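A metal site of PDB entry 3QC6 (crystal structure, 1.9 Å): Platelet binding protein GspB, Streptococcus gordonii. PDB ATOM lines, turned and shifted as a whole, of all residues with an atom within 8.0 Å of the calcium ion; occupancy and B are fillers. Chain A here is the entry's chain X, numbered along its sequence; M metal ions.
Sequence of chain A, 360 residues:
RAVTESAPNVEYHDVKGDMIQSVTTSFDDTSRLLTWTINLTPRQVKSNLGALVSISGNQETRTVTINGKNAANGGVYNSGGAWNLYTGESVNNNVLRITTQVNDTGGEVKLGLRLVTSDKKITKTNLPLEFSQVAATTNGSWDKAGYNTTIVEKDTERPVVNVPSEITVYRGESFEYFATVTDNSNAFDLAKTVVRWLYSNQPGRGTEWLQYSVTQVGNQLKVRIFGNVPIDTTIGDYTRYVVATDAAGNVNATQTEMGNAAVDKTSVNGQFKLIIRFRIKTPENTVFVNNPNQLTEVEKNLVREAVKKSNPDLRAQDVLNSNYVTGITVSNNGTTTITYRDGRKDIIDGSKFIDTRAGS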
ATOM      1  N   LYS A 154      11.727 -26.183  14.017  1.00  0.00           N
ATOM      2  CA  LYS A 154      11.836 -24.818  13.545  1.00  0.00           C
ATOM      3  C   LYS A 154      11.083 -23.903  14.509  1.00  0.00           C
ATOM      4  O   LYS A 154       9.886 -24.074  14.742  1.00  0.00           O
ATOM      5  CB  LYS A 154      11.295 -24.627  12.132  1.00  0.00           C
ATOM      6  CG  LYS A 154      11.683 -23.258  11.571  1.00  0.00           C
ATOM      7  CD  LYS A 154      11.062 -22.917  10.200  1.00  0.00           C
ATOM      8  CE  LYS A 154      11.538 -21.543   9.732  1.00  0.00           C
ATOM      9  NZ  LYS A 154      11.279 -21.304   8.287  1.00  0.00           N
ATOM     10  N   ASP A 155      11.798 -22.937  15.055  1.00  0.00           N
ATOM     11  CA  ASP A 155      11.206 -22.039  16.046  1.00  0.00           C
ATOM     12  C   ASP A 155      10.838 -20.708  15.403  1.00  0.00           C
ATOM     13  O   ASP A 155      11.720 -19.942  14.998  1.00  0.00           O
ATOM     14  CB  ASP A 155      12.161 -21.891  17.239  1.00  0.00           C
ATOM     15  CG  ASP A 155      11.627 -20.935  18.315  1.00  0.00           C
ATOM     16  OD1 ASP A 155      10.468 -20.474  18.224  1.00  0.00           O
ATOM     17  OD2 ASP A 155      12.415 -20.640  19.243  1.00  0.00           O
ATOM     18  N   THR A 156       9.530 -20.476  15.282  1.00  0.00           N
ATOM     19  CA  THR A 156       8.962 -19.256  14.723  1.00  0.00           C
ATOM     20  C   THR A 156       8.203 -18.421  15.762  1.00  0.00           C
ATOM     21  O   THR A 156       7.532 -17.446  15.413  1.00  0.00           O
ATOM     22  CB  THR A 156       7.999 -19.582  13.548  1.00  0.00           C
ATOM     23  OG1 THR A 156       6.897 -20.381  14.042  1.00  0.00           O
ATOM     24  CG2 THR A 156       8.749 -20.366  12.446  1.00  0.00           C
ATOM     25  N   GLU A 157       8.312 -18.780  17.043  1.00  0.00           N
ATOM     26  CA  GLU A 157       7.565 -18.060  18.099  1.00  0.00           C
ATOM     27  C   GLU A 157       8.512 -17.168  18.865  1.00  0.00           C
ATOM     28  O   GLU A 157       9.546 -17.623  19.330  1.00  0.00           O
ATOM     29  CB  GLU A 157       6.866 -19.057  19.060  1.00  0.00           C
ATOM     30  CG  GLU A 157       6.133 -18.399  20.291  1.00  0.00           C
ATOM     31  CD  GLU A 157       5.614 -19.458  21.258  1.00  0.00           C
ATOM     32  OE1 GLU A 157       5.197 -20.545  20.774  1.00  0.00           O
ATOM     33  OE2 GLU A 157       5.619 -19.217  22.502  1.00  0.00           O
ATOM     34  N   ARG A 158       8.160 -15.882  18.977  1.00  0.00           N
ATOM     35  CA  ARG A 158       9.032 -14.902  19.637  1.00  0.00           C
ATOM     36  C   ARG A 158       9.035 -15.112  21.153  1.00  0.00           C
ATOM     37  O   ARG A 158       8.018 -15.557  21.704  1.00  0.00           O
ATOM     38  CB  ARG A 158       8.502 -13.504  19.350  1.00  0.00           C
ATOM     39  CG  ARG A 158       8.525 -13.030  17.893  1.00  0.00           C
ATOM     40  CD  ARG A 158       7.877 -11.654  17.859  1.00  0.00           C
ATOM     41  NE  ARG A 158       7.858 -11.037  16.528  1.00  0.00           N
ATOM     42  CZ  ARG A 158       7.668  -9.741  16.325  1.00  0.00           C
ATOM     43  NH1 ARG A 158       7.562  -8.924  17.371  1.00  0.00           N
ATOM     44  NH2 ARG A 158       7.609  -9.251  15.084  1.00  0.00           N
ATOM     45  N   PRO A 159      10.178 -14.822  21.810  1.00  0.00           N
ATOM     46  CA  PRO A 159      10.345 -14.807  23.270  1.00  0.00           C
ATOM     47  C   PRO A 159       9.526 -13.699  23.877  1.00  0.00           C
ATOM     48  O   PRO A 159       9.213 -12.737  23.192  1.00  0.00           O
ATOM     49  CB  PRO A 159      11.839 -14.508  23.444  1.00  0.00           C
ATOM     50  CG  PRO A 159      12.194 -13.694  22.188  1.00  0.00           C
ATOM     51  CD  PRO A 159      11.430 -14.458  21.129  1.00  0.00           C
ATOM     52  N   VAL A 160       9.130 -13.865  25.136  1.00  0.00           N
ATOM     53  CA  VAL A 160       8.229 -12.914  25.757  1.00  0.00           C
ATOM     54  C   VAL A 160       8.889 -12.383  27.014  1.00  0.00           C
ATOM     55  O   VAL A 160       9.316 -13.165  27.890  1.00  0.00           O
ATOM     56  CB  VAL A 160       6.836 -13.533  26.140  1.00  0.00           C
ATOM     57  CG1 VAL A 160       5.954 -12.465  26.864  1.00  0.00           C
ATOM     58  CG2 VAL A 160       6.087 -14.114  24.880  1.00  0.00           C
ATOM     59  N   THR A 182      10.909 -15.455  28.760  1.00  0.00           N
ATOM     60  CA  THR A 182      10.654 -16.866  28.501  1.00  0.00           C
ATOM     61  C   THR A 182      10.572 -17.106  27.012  1.00  0.00           C
ATOM     62  O   THR A 182      10.408 -16.165  26.248  1.00  0.00           O
ATOM     63  CB  THR A 182       9.336 -17.303  29.138  1.00  0.00           C
ATOM     64  OG1 THR A 182       8.260 -16.559  28.568  1.00  0.00           O
ATOM     65  CG2 THR A 182       9.349 -17.072  30.651  1.00  0.00           C
ATOM     66  N   ASP A 183      10.715 -18.362  26.599  1.00  0.00           N
ATOM     67  CA  ASP A 183      10.552 -18.726  25.196  1.00  0.00           C
ATOM     68  C   ASP A 183      10.066 -20.175  25.088  1.00  0.00           C
ATOM     69  O   ASP A 183      10.468 -21.033  25.879  1.00  0.00           O
ATOM     70  CB  ASP A 183      11.871 -18.528  24.437  1.00  0.00           C
ATOM     71  CG  ASP A 183      11.695 -18.678  22.941  1.00  0.00           C
ATOM     72  OD1 ASP A 183      11.032 -17.828  22.333  1.00  0.00           O
ATOM     73  OD2 ASP A 183      12.172 -19.697  22.389  1.00  0.00           O
ATOM     74  N   ASN A 184       9.228 -20.448  24.090  1.00  0.00           N
ATOM     75  CA  ASN A 184       8.733 -21.790  23.830  1.00  0.00           C
ATOM     76  C   ASN A 184       9.869 -22.828  23.687  1.00  0.00           C
ATOM     77  O   ASN A 184       9.699 -24.012  24.040  1.00  0.00           O
ATOM     78  CB  ASN A 184       7.826 -21.796  22.574  1.00  0.00           C
ATOM     79  CG  ASN A 184       8.575 -21.419  21.297  1.00  0.00           C
ATOM     80  OD1 ASN A 184       9.170 -20.335  21.202  1.00  0.00           O
ATOM     81  ND2 ASN A 184       8.542 -22.320  20.289  1.00  0.00           N
ATOM     82  N   SER A 185      11.031 -22.386  23.191  1.00  0.00           N
ATOM     83  CA  SER A 185      12.180 -23.265  23.000  1.00  0.00           C
ATOM     84  C   SER A 185      13.012 -23.435  24.270  1.00  0.00           C
ATOM     85  O   SER A 185      13.854 -24.331  24.329  1.00  0.00           O
ATOM     86  CB  SER A 185      13.119 -22.740  21.895  1.00  0.00           C
ATOM     87  OG  SER A 185      13.935 -21.673  22.350  1.00  0.00           O
ATOM     88  N   ASN A 186      12.795 -22.546  25.242  1.00  0.00           N
ATOM     89  CA  ASN A 186      13.623 -22.465  26.441  1.00  0.00           C
ATOM     90  C   ASN A 186      15.113 -22.295  26.135  1.00  0.00           C
ATOM     91  O   ASN A 186      15.943 -22.571  27.011  1.00  0.00           O
ATOM     92  CB  ASN A 186      13.433 -23.685  27.339  1.00  0.00           C
ATOM     93  CG  ASN A 186      11.984 -23.914  27.738  1.00  0.00           C
ATOM     94  OD1 ASN A 186      11.251 -22.984  28.070  1.00  0.00           O
ATOM     95  ND2 ASN A 186      11.587 -25.150  27.736  1.00  0.00           N
ATOM     96  N   ALA A 187      15.434 -21.846  24.924  1.00  0.00           N
ATOM     97  CA  ALA A 187      16.821 -21.589  24.526  1.00  0.00           C
ATOM     98  C   ALA A 187      17.022 -20.182  23.946  1.00  0.00           C
ATOM     99  O   ALA A 187      16.318 -19.795  23.010  1.00  0.00           O
ATOM    100  CB  ALA A 187      17.348 -22.636  23.562  1.00  0.00           C
ATOM    101  N   PHE A 188      18.009 -19.478  24.482  1.00  0.00           N
ATOM    102  CA  PHE A 188      18.154 -18.023  24.256  1.00  0.00           C
ATOM    103  C   PHE A 188      19.490 -17.612  23.694  1.00  0.00           C
ATOM    104  O   PHE A 188      20.426 -18.423  23.681  1.00  0.00           O
ATOM    105  CB  PHE A 188      18.007 -17.292  25.576  1.00  0.00           C
ATOM    106  CG  PHE A 188      16.728 -17.570  26.298  1.00  0.00           C
ATOM    107  CD1 PHE A 188      15.583 -16.827  26.019  1.00  0.00           C
ATOM    108  CD2 PHE A 188      16.666 -18.559  27.280  1.00  0.00           C
ATOM    109  CE1 PHE A 188      14.377 -17.083  26.713  1.00  0.00           C
ATOM    110  CE2 PHE A 188      15.497 -18.799  27.987  1.00  0.00           C
ATOM    111  CZ  PHE A 188      14.348 -18.057  27.699  1.00  0.00           C
ATOM    112  N   THR A 245      16.308 -12.030  22.426  1.00  0.00           N
ATOM    113  CA  THR A 245      16.416 -12.834  21.218  1.00  0.00           C
ATOM    114  C   THR A 245      16.478 -14.287  21.638  1.00  0.00           C
ATOM    115  O   THR A 245      17.222 -14.623  22.555  1.00  0.00           O
ATOM    116  CB  THR A 245      17.720 -12.490  20.505  1.00  0.00           C
ATOM    117  OG1 THR A 245      17.746 -11.098  20.214  1.00  0.00           O
ATOM    118  CG2 THR A 245      17.900 -13.305  19.220  1.00  0.00           C
ATOM    119  N   ASP A 246      15.692 -15.153  20.982  1.00  0.00           N
ATOM    120  CA  ASP A 246      15.781 -16.571  21.325  1.00  0.00           C
ATOM    121  C   ASP A 246      16.937 -17.221  20.521  1.00  0.00           C
ATOM    122  O   ASP A 246      17.514 -16.586  19.646  1.00  0.00           O
ATOM    123  CB  ASP A 246      14.416 -17.271  21.170  1.00  0.00           C
ATOM    124  CG  ASP A 246      13.948 -17.387  19.751  1.00  0.00           C
ATOM    125  OD1 ASP A 246      14.742 -17.136  18.826  1.00  0.00           O
ATOM    126  OD2 ASP A 246      12.787 -17.734  19.540  1.00  0.00           O
ATOM    127  N   ALA A 247      17.322 -18.455  20.878  1.00  0.00           N
ATOM    128  CA  ALA A 247      18.381 -19.193  20.161  1.00  0.00           C
ATOM    129  C   ALA A 247      18.189 -19.186  18.630  1.00  0.00           C
ATOM    130  O   ALA A 247      19.169 -19.094  17.885  1.00  0.00           O
ATOM    131  CB  ALA A 247      18.486 -20.650  20.696  1.00  0.00           C
ATOM    132  N   ALA A 248      16.932 -19.289  18.180  1.00  0.00           N
ATOM    133  CA  ALA A 248      16.586 -19.296  16.759  1.00  0.00           C
ATOM    134  C   ALA A 248      16.716 -17.898  16.113  1.00  0.00           C
ATOM    135  O   ALA A 248      16.734 -17.779  14.910  1.00  0.00           O
ATOM    136  CB  ALA A 248      15.155 -19.850  16.539  1.00  0.00           C
ATOM    137  N   GLY A 249      16.795 -16.854  16.924  1.00  0.00           N
ATOM    138  CA  GLY A 249      16.979 -15.499  16.362  1.00  0.00           C
ATOM    139  C   GLY A 249      15.725 -14.642  16.371  1.00  0.00           C
ATOM    140  O   GLY A 249      15.751 -13.489  15.936  1.00  0.00           O
ATOM    141  N   ASN A 250      14.612 -15.194  16.844  1.00  0.00           N
ATOM    142  CA  ASN A 250      13.372 -14.399  17.005  1.00  0.00           C
ATOM    143  C   ASN A 250      13.537 -13.342  18.088  1.00  0.00           C
ATOM    144  O   ASN A 250      14.104 -13.627  19.147  1.00  0.00           O
ATOM    145  CB  ASN A 250      12.186 -15.299  17.379  1.00  0.00           C
ATOM    146  CG  ASN A 250      11.937 -16.394  16.378  1.00  0.00           C
ATOM    147  OD1 ASN A 250      12.044 -17.586  16.713  1.00  0.00           O
ATOM    148  ND2 ASN A 250      11.563 -16.022  15.142  1.00  0.00           N
ATOM    149  N   VAL A 251      13.016 -12.149  17.850  1.00  0.00           N
ATOM    150  CA  VAL A 251      13.057 -11.113  18.894  1.00  0.00           C
ATOM    151  C   VAL A 251      11.650 -10.778  19.374  1.00  0.00           C
ATOM    152  O   VAL A 251      10.702 -10.905  18.602  1.00  0.00           O
ATOM    153  CB  VAL A 251      13.798  -9.819  18.416  1.00  0.00           C
ATOM    154  CG1 VAL A 251      15.277 -10.093  18.262  1.00  0.00           C
ATOM    155  CG2 VAL A 251      13.204  -9.259  17.135  1.00  0.00           C
HETATM  156 CA    CA M   1      10.908 -19.043  20.327  1.00  0.00          CA
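The calcium ion is bound by the backbone carbonyl oxygen (O) of Glu 157 (2.2 Å), the side-chain amide oxygen (OD1) of Asn 184 (2.3 Å), the side-chain carboxylate (OD1) of Asp 183 (2.3 Å), the side-chain carboxylate (OD2) of Asp 246 (2.4 Å), the side-chain carboxylate (OD2) of Asp 155 (2.4 Å), the side-chain carboxylate (OD2) of Asp 183 (2.5 Å) and the side-chain carboxylate (OD1) of Asp 155 (2.6 Å). The calcium ion has seven donor atoms within binding distance.
The side-chain carboxylate (OD2) of Asp 183 sits close to the side-chain hydroxyl (OG) of Ser 185 (2.6 Å). The side-chain amide oxygen (OD1) of Asn 186 sits close to the backbone carbonyl oxygen (O) of Asp 183 (3.0 Å). OD1 of Asp 246 lies within hydrogen-bond range of N of Asn 250 (2.8 Å). OD1 of Asp 246 lies close to N of Ala 248, at 3.1 Å. OD1 of Asp 246 lies within hydrogen-bond range of N of Gly 249. The backbone carbonyl oxygen of Asp 155 lies close to the side-chain amide oxygen of Asn 250, 2.9 Å away.
Within 4 Å of the calcium ion: Asp 155, Glu 157, Asp 183, Asn 184 and Asp 246.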
